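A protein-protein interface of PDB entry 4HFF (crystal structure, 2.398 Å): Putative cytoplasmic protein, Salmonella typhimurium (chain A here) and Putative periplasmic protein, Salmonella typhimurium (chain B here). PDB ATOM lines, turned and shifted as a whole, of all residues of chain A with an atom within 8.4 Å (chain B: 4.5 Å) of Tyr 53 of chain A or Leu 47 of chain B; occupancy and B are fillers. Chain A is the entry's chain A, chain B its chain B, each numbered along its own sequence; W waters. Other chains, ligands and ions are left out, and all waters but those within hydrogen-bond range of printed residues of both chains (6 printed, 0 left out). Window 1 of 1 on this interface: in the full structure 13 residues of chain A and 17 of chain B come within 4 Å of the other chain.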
ATOM      1  N   VAL A  34     -35.569  29.838 -30.166  1.00  0.00           N
ATOM      2  CA  VAL A  34     -34.523  28.875 -30.497  1.00  0.00           C
ATOM      3  C   VAL A  34     -34.570  28.477 -31.974  1.00  0.00           C
ATOM      4  O   VAL A  34     -33.527  28.283 -32.602  1.00  0.00           O
ATOM      5  CB  VAL A  34     -34.552  27.631 -29.560  1.00  0.00           C
ATOM      6  CG1 VAL A  34     -35.906  26.881 -29.647  1.00  0.00           C
ATOM      7  CG2 VAL A  34     -33.373  26.705 -29.862  1.00  0.00           C
ATOM      8  N   ASN A  44     -24.609  22.946 -38.329  1.00  0.00           N
ATOM      9  CA  ASN A  44     -24.992  21.927 -37.357  1.00  0.00           C
ATOM     10  C   ASN A  44     -25.834  22.450 -36.193  1.00  0.00           C
ATOM     11  O   ASN A  44     -26.632  21.701 -35.614  1.00  0.00           O
ATOM     12  CB  ASN A  44     -23.760  21.168 -36.864  1.00  0.00           C
ATOM     13  CG  ASN A  44     -23.195  20.259 -37.928  1.00  0.00           C
ATOM     14  OD1 ASN A  44     -23.906  19.869 -38.864  1.00  0.00           O
ATOM     15  ND2 ASN A  44     -21.922  19.910 -37.800  1.00  0.00           N
ATOM     16  N   VAL A  45     -25.664  23.726 -35.851  1.00  0.00           N
ATOM     17  CA  VAL A  45     -26.525  24.350 -34.849  1.00  0.00           C
ATOM     18  C   VAL A  45     -27.974  24.320 -35.339  1.00  0.00           C
ATOM     19  O   VAL A  45     -28.867  23.774 -34.661  1.00  0.00           O
ATOM     20  CB  VAL A  45     -26.119  25.807 -34.571  1.00  0.00           C
ATOM     21  CG1 VAL A  45     -27.125  26.477 -33.636  1.00  0.00           C
ATOM     22  CG2 VAL A  45     -24.706  25.870 -34.005  1.00  0.00           C
ATOM     23  N   GLY A  46     -28.184  24.895 -36.525  1.00  0.00           N
ATOM     24  CA  GLY A  46     -29.493  24.934 -37.151  1.00  0.00           C
ATOM     25  C   GLY A  46     -30.075  23.543 -37.312  1.00  0.00           C
ATOM     26  O   GLY A  46     -31.263  23.338 -37.107  1.00  0.00           O
ATOM     27  N   LYS A  47     -29.225  22.587 -37.668  1.00  0.00           N
ATOM     28  CA  LYS A  47     -29.642  21.216 -37.906  1.00  0.00           C
ATOM     29  C   LYS A  47     -30.130  20.567 -36.611  1.00  0.00           C
ATOM     30  O   LYS A  47     -31.190  19.929 -36.592  1.00  0.00           O
ATOM     31  CB  LYS A  47     -28.477  20.426 -38.515  1.00  0.00           C
ATOM     32  CG  LYS A  47     -28.789  18.975 -38.827  1.00  0.00           C
ATOM     33  N   ASN A  48     -29.376  20.744 -35.530  1.00  0.00           N
ATOM     34  CA  ASN A  48     -29.788  20.180 -34.248  1.00  0.00           C
ATOM     35  C   ASN A  48     -31.040  20.841 -33.673  1.00  0.00           C
ATOM     36  O   ASN A  48     -31.847  20.177 -33.015  1.00  0.00           O
ATOM     37  CB  ASN A  48     -28.640  20.202 -33.240  1.00  0.00           C
ATOM     38  CG  ASN A  48     -27.645  19.092 -33.484  1.00  0.00           C
ATOM     39  OD1 ASN A  48     -27.852  17.956 -33.044  1.00  0.00           O
ATOM     40  ND2 ASN A  48     -26.546  19.413 -34.179  1.00  0.00           N
ATOM     41  N   ILE A  49     -31.200  22.141 -33.921  1.00  0.00           N
ATOM     42  CA  ILE A  49     -32.413  22.846 -33.502  1.00  0.00           C
ATOM     43  C   ILE A  49     -33.630  22.375 -34.312  1.00  0.00           C
ATOM     44  O   ILE A  49     -34.708  22.139 -33.752  1.00  0.00           O
ATOM     45  CB  ILE A  49     -32.238  24.386 -33.592  1.00  0.00           C
ATOM     46  CG1 ILE A  49     -31.381  24.866 -32.411  1.00  0.00           C
ATOM     47  CG2 ILE A  49     -33.596  25.089 -33.625  1.00  0.00           C
ATOM     48  CD1 ILE A  49     -30.873  26.301 -32.512  1.00  0.00           C
ATOM     49  N   THR A  50     -33.445  22.223 -35.622  1.00  0.00           N
ATOM     50  CA  THR A  50     -34.486  21.716 -36.511  1.00  0.00           C
ATOM     51  C   THR A  50     -34.985  20.350 -36.035  1.00  0.00           C
ATOM     52  O   THR A  50     -36.199  20.090 -36.011  1.00  0.00           O
ATOM     53  CB  THR A  50     -33.964  21.595 -37.970  1.00  0.00           C
ATOM     54  OG1 THR A  50     -33.809  22.902 -38.549  1.00  0.00           O
ATOM     55  CG2 THR A  50     -34.928  20.787 -38.824  1.00  0.00           C
ATOM     56  N   GLY A  51     -34.046  19.488 -35.646  1.00  0.00           N
ATOM     57  CA  GLY A  51     -34.373  18.156 -35.172  1.00  0.00           C
ATOM     58  C   GLY A  51     -34.899  18.129 -33.745  1.00  0.00           C
ATOM     59  O   GLY A  51     -35.273  17.059 -33.251  1.00  0.00           O
ATOM     60  N   GLY A  52     -34.935  19.287 -33.080  1.00  0.00           N
ATOM     61  CA  GLY A  52     -35.449  19.369 -31.716  1.00  0.00           C
ATOM     62  C   GLY A  52     -34.483  18.958 -30.604  1.00  0.00           C
ATOM     63  O   GLY A  52     -34.865  18.946 -29.429  1.00  0.00           O
ATOM     64  N   TYR A  53     -33.242  18.618 -30.966  1.00  0.00           N
ATOM     65  CA  TYR A  53     -32.244  18.169 -29.987  1.00  0.00           C
ATOM     66  C   TYR A  53     -31.841  19.303 -29.057  1.00  0.00           C
ATOM     67  O   TYR A  53     -31.487  19.075 -27.894  1.00  0.00           O
ATOM     68  CB  TYR A  53     -30.982  17.638 -30.688  1.00  0.00           C
ATOM     69  CG  TYR A  53     -31.213  16.453 -31.599  1.00  0.00           C
ATOM     70  CD1 TYR A  53     -31.098  15.149 -31.124  1.00  0.00           C
ATOM     71  CD2 TYR A  53     -31.534  16.629 -32.941  1.00  0.00           C
ATOM     72  CE1 TYR A  53     -31.311  14.048 -31.967  1.00  0.00           C
ATOM     73  CE2 TYR A  53     -31.750  15.535 -33.788  1.00  0.00           C
ATOM     74  CZ  TYR A  53     -31.642  14.248 -33.289  1.00  0.00           C
ATOM     75  OH  TYR A  53     -31.852  13.165 -34.116  1.00  0.00           O
ATOM     76  N   PHE A  54     -31.843  20.520 -29.594  1.00  0.00           N
ATOM     77  CA  PHE A  54     -31.499  21.702 -28.809  1.00  0.00           C
ATOM     78  C   PHE A  54     -32.762  22.542 -28.578  1.00  0.00           C
ATOM     79  O   PHE A  54     -33.430  22.942 -29.536  1.00  0.00           O
ATOM     80  CB  PHE A  54     -30.418  22.534 -29.526  1.00  0.00           C
ATOM     81  CG  PHE A  54     -29.072  21.830 -29.666  1.00  0.00           C
ATOM     82  CD1 PHE A  54     -28.778  20.677 -28.937  1.00  0.00           C
ATOM     83  CD2 PHE A  54     -28.085  22.347 -30.511  1.00  0.00           C
ATOM     84  CE1 PHE A  54     -27.533  20.040 -29.054  1.00  0.00           C
ATOM     85  CE2 PHE A  54     -26.843  21.718 -30.636  1.00  0.00           C
ATOM     86  CZ  PHE A  54     -26.566  20.564 -29.911  1.00  0.00           C
ATOM     87  N   GLN A  55     -33.093  22.808 -27.316  1.00  0.00           N
ATOM     88  CA  GLN A  55     -34.280  23.598 -27.004  1.00  0.00           C
ATOM     89  C   GLN A  55     -33.923  24.819 -26.164  1.00  0.00           C
ATOM     90  O   GLN A  55     -34.643  25.827 -26.173  1.00  0.00           O
ATOM     91  CB  GLN A  55     -35.347  22.730 -26.295  1.00  0.00           C
ATOM     92  CG  GLN A  55     -35.945  21.614 -27.166  1.00  0.00           C
ATOM     93  CD  GLN A  55     -36.819  22.142 -28.308  1.00  0.00           C
ATOM     94  OE1 GLN A  55     -36.467  22.031 -29.488  1.00  0.00           O
ATOM     95  NE2 GLN A  55     -37.967  22.697 -27.959  1.00  0.00           N
ATOM     96  N   ASN A  56     -32.812  24.719 -25.438  1.00  0.00           N
ATOM     97  CA  ASN A  56     -32.316  25.831 -24.626  1.00  0.00           C
ATOM     98  C   ASN A  56     -31.242  26.624 -25.387  1.00  0.00           C
ATOM     99  O   ASN A  56     -30.093  26.182 -25.492  1.00  0.00           O
ATOM    100  CB  ASN A  56     -31.731  25.308 -23.311  1.00  0.00           C
ATOM    101  CG  ASN A  56     -31.464  26.418 -22.301  1.00  0.00           C
ATOM    102  OD1 ASN A  56     -31.514  27.608 -22.631  1.00  0.00           O
ATOM    103  ND2 ASN A  56     -31.173  26.027 -21.056  1.00  0.00           N
ATOM    104  N   PRO A  59     -26.857  28.825 -23.885  1.00  0.00           N
ATOM    105  CA  PRO A  59     -25.413  28.712 -24.132  1.00  0.00           C
ATOM    106  C   PRO A  59     -25.090  28.985 -25.600  1.00  0.00           C
ATOM    107  O   PRO A  59     -24.010  29.488 -25.929  1.00  0.00           O
ATOM    108  CB  PRO A  59     -25.102  27.251 -23.771  1.00  0.00           C
ATOM    109  CG  PRO A  59     -26.406  26.517 -24.013  1.00  0.00           C
ATOM    110  CD  PRO A  59     -27.474  27.507 -23.615  1.00  0.00           C
ATOM    111  N   ILE A  60     -26.026  28.664 -26.485  1.00  0.00           N
ATOM    112  CA  ILE A  60     -25.796  28.940 -27.898  1.00  0.00           C
ATOM    113  C   ILE A  60     -25.728  30.445 -28.165  1.00  0.00           C
ATOM    114  O   ILE A  60     -24.837  30.927 -28.888  1.00  0.00           O
ATOM    115  CB  ILE A  60     -26.851  28.264 -28.777  1.00  0.00           C
ATOM    116  CG1 ILE A  60     -26.729  26.742 -28.613  1.00  0.00           C
ATOM    117  CG2 ILE A  60     -26.677  28.682 -30.230  1.00  0.00           C
ATOM    118  CD1 ILE A  60     -27.850  25.956 -29.241  1.00  0.00           C
ATOM    119  N   ALA A  80     -18.542  20.256 -25.076  1.00  0.00           N
ATOM    120  CA  ALA A  80     -19.338  19.808 -26.214  1.00  0.00           C
ATOM    121  C   ALA A  80     -19.755  20.996 -27.097  1.00  0.00           C
ATOM    122  O   ALA A  80     -20.411  21.939 -26.625  1.00  0.00           O
ATOM    123  CB  ALA A  80     -20.566  19.023 -25.733  1.00  0.00           C
ATOM    124  N   TYR A  92     -23.531  23.916 -26.260  1.00  0.00           N
ATOM    125  CA  TYR A  92     -24.980  23.741 -26.174  1.00  0.00           C
ATOM    126  C   TYR A  92     -25.518  23.380 -24.789  1.00  0.00           C
ATOM    127  O   TYR A  92     -26.730  23.232 -24.615  1.00  0.00           O
ATOM    128  CB  TYR A  92     -25.489  22.778 -27.260  1.00  0.00           C
ATOM    129  CG  TYR A  92     -24.829  21.411 -27.288  1.00  0.00           C
ATOM    130  CD1 TYR A  92     -25.344  20.357 -26.550  1.00  0.00           C
ATOM    131  CD2 TYR A  92     -23.714  21.164 -28.087  1.00  0.00           C
ATOM    132  CE1 TYR A  92     -24.764  19.091 -26.586  1.00  0.00           C
ATOM    133  CE2 TYR A  92     -23.129  19.899 -28.129  1.00  0.00           C
ATOM    134  CZ  TYR A  92     -23.667  18.863 -27.372  1.00  0.00           C
ATOM    135  OH  TYR A  92     -23.102  17.603 -27.382  1.00  0.00           O
ATOM    136  N   ARG A  93     -24.626  23.283 -23.804  1.00  0.00           N
ATOM    137  CA  ARG A  93     -25.025  22.986 -22.428  1.00  0.00           C
ATOM    138  C   ARG A  93     -24.694  24.170 -21.525  1.00  0.00           C
ATOM    139  O   ARG A  93     -23.582  24.716 -21.584  1.00  0.00           O
ATOM    140  CB  ARG A  93     -24.322  21.711 -21.918  1.00  0.00           C
ATOM    141  CG  ARG A  93     -24.709  20.411 -22.659  1.00  0.00           C
ATOM    142  CD  ARG A  93     -24.069  19.176 -22.009  1.00  0.00           C
ATOM    143  NE  ARG A  93     -24.716  17.933 -22.433  1.00  0.00           N
ATOM    144  CZ  ARG A  93     -24.167  17.033 -23.248  1.00  0.00           C
ATOM    145  NH1 ARG A  93     -22.934  17.219 -23.703  1.00  0.00           N
ATOM    146  NH2 ARG A  93     -24.842  15.933 -23.595  1.00  0.00           N
ATOM    147  N   VAL A  94     -25.659  24.560 -20.696  1.00  0.00           N
ATOM    148  CA  VAL A  94     -25.481  25.663 -19.765  1.00  0.00           C
ATOM    149  C   VAL A  94     -24.252  25.459 -18.868  1.00  0.00           C
ATOM    150  O   VAL A  94     -23.402  26.363 -18.750  1.00  0.00           O
ATOM    151  CB  VAL A  94     -26.754  25.894 -18.915  1.00  0.00           C
ATOM    152  CG1 VAL A  94     -26.520  26.960 -17.830  1.00  0.00           C
ATOM    153  CG2 VAL A  94     -27.924  26.294 -19.810  1.00  0.00           C
ATOM    154  N   ASP A  96     -21.582  23.679 -19.341  1.00  0.00           N
ATOM    155  CA  ASP A  96     -20.372  23.827 -20.145  1.00  0.00           C
ATOM    156  C   ASP A  96     -20.067  25.297 -20.386  1.00  0.00           C
ATOM    157  O   ASP A  96     -18.924  25.717 -20.256  1.00  0.00           O
ATOM    158  CB  ASP A  96     -20.489  23.107 -21.497  1.00  0.00           C
ATOM    159  CG  ASP A  96     -20.228  21.603 -21.404  1.00  0.00           C
ATOM    160  OD1 ASP A  96     -19.725  21.126 -20.362  1.00  0.00           O
ATOM    161  OD2 ASP A  96     -20.512  20.901 -22.400  1.00  0.00           O
ATOM    162  N   ASN A 136     -34.579  21.900 -15.938  1.00  0.00           N
ATOM    163  CA  ASN A 136     -33.816  21.678 -17.168  1.00  0.00           C
ATOM    164  C   ASN A 136     -32.378  22.192 -17.086  1.00  0.00           C
ATOM    165  O   ASN A 136     -31.623  22.041 -18.038  1.00  0.00           O
ATOM    166  CB  ASN A 136     -34.509  22.350 -18.352  1.00  0.00           C
ATOM    167  CG  ASN A 136     -34.439  23.872 -18.268  1.00  0.00           C
ATOM    168  OD1 ASN A 136     -34.773  24.464 -17.236  1.00  0.00           O
ATOM    169  ND2 ASN A 136     -33.971  24.506 -19.340  1.00  0.00           N
ATOM    170  N   TRP B  20     -34.037  10.256 -22.054  1.00  0.00           N
ATOM    171  CA  TRP B  20     -33.941  10.995 -23.305  1.00  0.00           C
ATOM    172  C   TRP B  20     -34.583  10.192 -24.423  1.00  0.00           C
ATOM    173  O   TRP B  20     -35.375  10.722 -25.192  1.00  0.00           O
ATOM    174  CB  TRP B  20     -32.476  11.329 -23.697  1.00  0.00           C
ATOM    175  CG  TRP B  20     -32.452  12.350 -24.820  1.00  0.00           C
ATOM    176  CD1 TRP B  20     -32.387  13.711 -24.683  1.00  0.00           C
ATOM    177  CD2 TRP B  20     -32.560  12.100 -26.225  1.00  0.00           C
ATOM    178  NE1 TRP B  20     -32.435  14.315 -25.911  1.00  0.00           N
ATOM    179  CE2 TRP B  20     -32.550  13.341 -26.890  1.00  0.00           C
ATOM    180  CE3 TRP B  20     -32.665  10.936 -27.008  1.00  0.00           C
ATOM    181  CZ2 TRP B  20     -32.633  13.477 -28.279  1.00  0.00           C
ATOM    182  CZ3 TRP B  20     -32.752  11.059 -28.395  1.00  0.00           C
ATOM    183  CH2 TRP B  20     -32.732  12.324 -29.017  1.00  0.00           C
ATOM    184  N   ALA B  43     -36.880  16.133 -23.111  1.00  0.00           N
ATOM    185  CA  ALA B  43     -35.673  15.526 -23.661  1.00  0.00           C
ATOM    186  C   ALA B  43     -34.467  16.462 -23.484  1.00  0.00           C
ATOM    187  O   ALA B  43     -33.396  16.029 -23.011  1.00  0.00           O
ATOM    188  CB  ALA B  43     -35.868  15.166 -25.147  1.00  0.00           C
ATOM    189  N   SER B  44     -34.655  17.739 -23.842  1.00  0.00           N
ATOM    190  CA  SER B  44     -33.557  18.711 -23.789  1.00  0.00           C
ATOM    191  C   SER B  44     -33.031  18.803 -22.368  1.00  0.00           C
ATOM    192  O   SER B  44     -31.819  18.894 -22.169  1.00  0.00           O
ATOM    193  CB  SER B  44     -33.966  20.091 -24.322  1.00  0.00           C
ATOM    194  OG  SER B  44     -34.651  20.846 -23.338  1.00  0.00           O
ATOM    195  N   ALA B  45     -33.927  18.719 -21.382  1.00  0.00           N
ATOM    196  CA  ALA B  45     -33.465  18.673 -19.992  1.00  0.00           C
ATOM    197  C   ALA B  45     -32.509  17.514 -19.769  1.00  0.00           C
ATOM    198  O   ALA B  45     -31.450  17.690 -19.143  1.00  0.00           O
ATOM    199  CB  ALA B  45     -34.612  18.587 -19.025  1.00  0.00           C
ATOM    200  N   TYR B  46     -32.865  16.335 -20.282  1.00  0.00           N
ATOM    201  CA  TYR B  46     -31.972  15.190 -20.052  1.00  0.00           C
ATOM    202  C   TYR B  46     -30.649  15.302 -20.816  1.00  0.00           C
ATOM    203  O   TYR B  46     -29.616  14.776 -20.384  1.00  0.00           O
ATOM    204  CB  TYR B  46     -32.676  13.862 -20.347  1.00  0.00           C
ATOM    205  CG  TYR B  46     -33.885  13.683 -19.465  1.00  0.00           C
ATOM    206  CD1 TYR B  46     -33.760  13.723 -18.075  1.00  0.00           C
ATOM    207  CD2 TYR B  46     -35.155  13.507 -20.010  1.00  0.00           C
ATOM    208  CE1 TYR B  46     -34.867  13.580 -17.253  1.00  0.00           C
ATOM    209  CE2 TYR B  46     -36.272  13.354 -19.184  1.00  0.00           C
ATOM    210  CZ  TYR B  46     -36.115  13.396 -17.812  1.00  0.00           C
ATOM    211  OH  TYR B  46     -37.196  13.263 -16.983  1.00  0.00           O
ATOM    212  N   LEU B  47     -30.682  15.982 -21.954  1.00  0.00           N
ATOM    213  CA  LEU B  47     -29.472  16.204 -22.732  1.00  0.00           C
ATOM    214  C   LEU B  47     -28.552  17.189 -22.011  1.00  0.00           C
ATOM    215  O   LEU B  47     -27.327  17.034 -22.042  1.00  0.00           O
ATOM    216  CB  LEU B  47     -29.830  16.715 -24.133  1.00  0.00           C
ATOM    217  CG  LEU B  47     -28.679  17.017 -25.094  1.00  0.00           C
ATOM    218  CD1 LEU B  47     -29.047  16.593 -26.507  1.00  0.00           C
ATOM    219  CD2 LEU B  47     -28.305  18.508 -25.060  1.00  0.00           C
ATOM    220  N   GLU B  48     -29.146  18.185 -21.350  1.00  0.00           N
ATOM    221  CA  GLU B  48     -28.375  19.188 -20.615  1.00  0.00           C
ATOM    222  C   GLU B  48     -27.430  18.544 -19.603  1.00  0.00           C
ATOM    223  O   GLU B  48     -26.264  18.937 -19.490  1.00  0.00           O
ATOM    224  CB  GLU B  48     -29.315  20.179 -19.909  1.00  0.00           C
ATOM    225  CG  GLU B  48     -28.672  20.967 -18.760  1.00  0.00           C
ATOM    226  CD  GLU B  48     -27.603  21.985 -19.244  1.00  0.00           C
ATOM    227  OE1 GLU B  48     -27.764  22.535 -20.363  1.00  0.00           O
ATOM    228  OE2 GLU B  48     -26.616  22.258 -18.503  1.00  0.00           O
ATOM    229  N   TYR B  49     -27.919  17.533 -18.894  1.00  0.00           N
ATOM    230  CA  TYR B  49     -27.119  16.921 -17.833  1.00  0.00           C
ATOM    231  C   TYR B  49     -26.254  15.763 -18.318  1.00  0.00           C
ATOM    232  O   TYR B  49     -25.502  15.169 -17.531  1.00  0.00           O
ATOM    233  CB  TYR B  49     -28.017  16.487 -16.662  1.00  0.00           C
ATOM    234  CG  TYR B  49     -28.634  17.668 -15.936  1.00  0.00           C
ATOM    235  CD1 TYR B  49     -27.910  18.385 -14.996  1.00  0.00           C
ATOM    236  CD2 TYR B  49     -29.929  18.083 -16.208  1.00  0.00           C
ATOM    237  CE1 TYR B  49     -28.469  19.477 -14.336  1.00  0.00           C
ATOM    238  CE2 TYR B  49     -30.494  19.183 -15.549  1.00  0.00           C
ATOM    239  CZ  TYR B  49     -29.757  19.866 -14.610  1.00  0.00           C
ATOM    240  OH  TYR B  49     -30.293  20.948 -13.942  1.00  0.00           O
ATOM    241  N   GLY B  50     -26.364  15.437 -19.607  1.00  0.00           N
ATOM    242  CA  GLY B  50     -25.526  14.403 -20.201  1.00  0.00           C
ATOM    243  C   GLY B  50     -24.071  14.846 -20.380  1.00  0.00           C
ATOM    244  O   GLY B  50     -23.773  16.055 -20.435  1.00  0.00           O
ATOM    245  N   TYR B  57     -27.187  10.945 -29.322  1.00  0.00           N
ATOM    246  CA  TYR B  57     -28.596  11.280 -29.415  1.00  0.00           C
ATOM    247  C   TYR B  57     -29.093  11.103 -30.845  1.00  0.00           C
ATOM    248  O   TYR B  57     -30.211  10.626 -31.063  1.00  0.00           O
ATOM    249  CB  TYR B  57     -28.848  12.704 -28.913  1.00  0.00           C
ATOM    250  CG  TYR B  57     -28.349  12.924 -27.506  1.00  0.00           C
ATOM    251  CD1 TYR B  57     -29.100  12.515 -26.399  1.00  0.00           C
ATOM    252  CD2 TYR B  57     -27.126  13.531 -27.276  1.00  0.00           C
ATOM    253  CE1 TYR B  57     -28.630  12.717 -25.097  1.00  0.00           C
ATOM    254  CE2 TYR B  57     -26.650  13.743 -25.987  1.00  0.00           C
ATOM    255  CZ  TYR B  57     -27.394  13.337 -24.907  1.00  0.00           C
ATOM    256  OH  TYR B  57     -26.892  13.555 -23.644  1.00  0.00           O
ATOM    257  N   HIS B  58     -28.277  11.477 -31.826  1.00  0.00           N
ATOM    258  CA  HIS B  58     -28.660  11.177 -33.215  1.00  0.00           C
ATOM    259  C   HIS B  58     -28.884   9.675 -33.447  1.00  0.00           C
ATOM    260  O   HIS B  58     -29.801   9.276 -34.182  1.00  0.00           O
ATOM    261  CB  HIS B  58     -27.614  11.701 -34.201  1.00  0.00           C
ATOM    262  CG  HIS B  58     -27.438  13.185 -34.150  1.00  0.00           C
ATOM    263  ND1 HIS B  58     -26.403  13.835 -34.791  1.00  0.00           N
ATOM    264  CD2 HIS B  58     -28.168  14.149 -33.538  1.00  0.00           C
ATOM    265  CE1 HIS B  58     -26.504  15.133 -34.574  1.00  0.00           C
ATOM    266  NE2 HIS B  58     -27.563  15.351 -33.814  1.00  0.00           N
ATOM    267  N   ASP B  61     -31.949   8.448 -31.934  1.00  0.00           N
ATOM    268  CA  ASP B  61     -33.018   8.822 -32.851  1.00  0.00           C
ATOM    269  C   ASP B  61     -33.173   7.855 -34.020  1.00  0.00           C
ATOM    270  O   ASP B  61     -34.297   7.569 -34.427  1.00  0.00           O
ATOM    271  CB  ASP B  61     -32.833  10.247 -33.371  1.00  0.00           C
ATOM    272  CG  ASP B  61     -33.826  10.594 -34.474  1.00  0.00           C
ATOM    273  OD1 ASP B  61     -34.980  10.961 -34.143  1.00  0.00           O
ATOM    274  OD2 ASP B  61     -33.462  10.500 -35.675  1.00  0.00           O
HETATM  275  O   HOH W   1     -33.010  22.478 -21.470  1.00  0.00           O
HETATM  276  O   HOH W   2     -28.279  21.712 -22.802  1.00  0.00           O
HETATM  277  O   HOH W   3     -30.524  23.436 -20.311  1.00  0.00           O
HETATM  278  O   HOH W   4     -32.734  16.975 -26.294  1.00  0.00           O
HETATM  279  O   HOH W   5     -32.733  20.631 -13.301  1.00  0.00           O
HETATM  280  O   HOH W   6     -35.799  14.287 -34.837  1.00  0.00           O
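The backbone carbonyl oxygen (O) of Gly 50 of chain B is in hydrogen-bond range of the guanidinium group (NE) of Arg 93 of chain A (2.9 Å).
NH2 of Arg 93 of chain A lies within hydrogen-bond range of OH of Tyr 57 of chain B (3.1 Å).
The side-chain carboxylate (OD2) of Asp 61 of chain B sits close to the side-chain hydroxyl (OH) of Tyr 53 of chain A, 3.5 Å away.
N of Val 94 of chain A lies within hydrogen-bond range of OE1 of Glu 48 of chain B (2.9 Å).
NE of Arg 93 of chain A is in hydrogen-bond range of O of Leu 47 of chain B, at 2.8 Å.
The guanidinium group (NE) of Arg 93 of chain A sits close to the backbone carbonyl oxygen (O) of Glu 48 of chain B (3.5 Å).
The side-chain amide oxygen (OD1) of Asn 48 of chain A sits at hydrogen-bond distance from a ring nitrogen (NE2) of His 58 of chain B, at 2.7 Å.
O of Asn 48 of chain A is in hydrogen-bond range of N of Tyr 53 of chain A (2.9 Å).
The backbone NH (N) of Phe 54 of chain A lies within hydrogen-bond range of the backbone carbonyl oxygen (O) of Asn 48 of chain A (3.4 Å).
OE1 of Gln 55 of chain A lies close to O of Gly 52 of chain A, at 3.5 Å.
The backbone carbonyl oxygen (O) of Asn 44 of chain A sits at hydrogen-bond distance from the side-chain amide nitrogen (ND2) of Asn 48 of chain A (2.7 Å).
Among the printed residues, merely in contact across the chains: Asn 136 of chain A with Glu 48 of chain B (3.2 Å), Tyr 53 of chain A with His 58 of chain B (3.5 Å), Gln 55 of chain A with Ser 44 of chain B (3.6 Å), Tyr 53 of chain A with Trp 20 of chain B (3.6 Å), Asn 136 of chain A with Ala 45 of chain B (3.7 Å), Tyr 53 of chain A with Tyr 57 of chain B (3.7 Å), Tyr 53 of chain A with Leu 47 of chain B (3.7 Å), Tyr 92 of chain A with Leu 47 of chain B (3.8 Å) and Asn 136 of chain A with Tyr 49 of chain B (3.9 Å).
Of chain B, only Trp 20, Leu 47, Tyr 57, His 58 and Asp 61 come within 4 Å of Tyr 53 of chain A.
Printed residues of chain B within 4 Å of Gln 55 of chain A: Ser 44 (3.6 Å).
Of the printed residues of chain A, Trp 20 of chain B touches Tyr 53 (3.6 Å).
Leu 47 of chain B touches just these residues of chain A: Tyr 53 (3.7 Å), Tyr 92 (3.8 Å) and Arg 93 (2.8 Å).
Printed residues of chain A within 4 Å of Tyr 49 of chain B: Asn 136.
Gly 50 of chain B touches just one residue of chain A: Arg 93 (2.9 Å).
Of the printed residues of chain A, His 58 of chain B touches Asn 48 (2.7 Å) and Tyr 53 (3.5 Å).
The nearest printed residue of chain B that does not touch Arg 93 of chain A is Tyr 49 of chain B (4.8 Å).
Of the 12 printed residues of chain B, 10 touch a printed residue of chain A.
Printed residues of chain B that touch a printed residue of chain A: Trp 20, Ser 44, Ala 45, Leu 47, Glu 48, Tyr 49, Gly 50, Tyr 57, His 58 and Asp 61.
Hydrophobic or aromatic side chains of chain B within 4 Å of the printed part of chain A: Trp 20, Ala 45, Leu 47, Tyr 49, Tyr 57 and His 58.
Of the 22 printed residues of chain A, 7 touch a printed residue of chain B.
Among the printed residues, 16 pairs touch across the chains.
Water W5 bridges the side-chain hydroxyl (OH) of Tyr 49 of chain B and the backbone NH (N) of Asn 136 of chain A.
Water W2 lies within hydrogen-bond range of the side-chain carboxylate (OE1) of Glu 48 of chain B (2.6 Å) and the backbone carbonyl oxygen (O) of Tyr 92 of chain A (2.8 Å).
Water W4 lies within hydrogen-bond range of NE1 of Trp 20 of chain B (2.7 Å), O of Tyr 53 of chain A (2.9 Å), N of Ser 44 of chain B (3.2 Å) and O of Ala 43 of chain B (3.5 Å).
Water W3 lies within hydrogen-bond range of the side-chain amide nitrogen of Asn 56 of chain A (2.8 Å), the backbone carbonyl oxygen of Asn 136 of chain A (2.9 Å) and the side-chain carboxylate of Glu 48 of chain B (2.9 Å).
Water W1 bridges OG of Ser 44 of chain B (3.0 Å) and ND2 of Asn 136 of chain A (3.1 Å).
Water W6 lies within hydrogen-bond range of the backbone carbonyl oxygen of Gly 51 of chain A and the side-chain carboxylate of Asp 61 of chain B.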
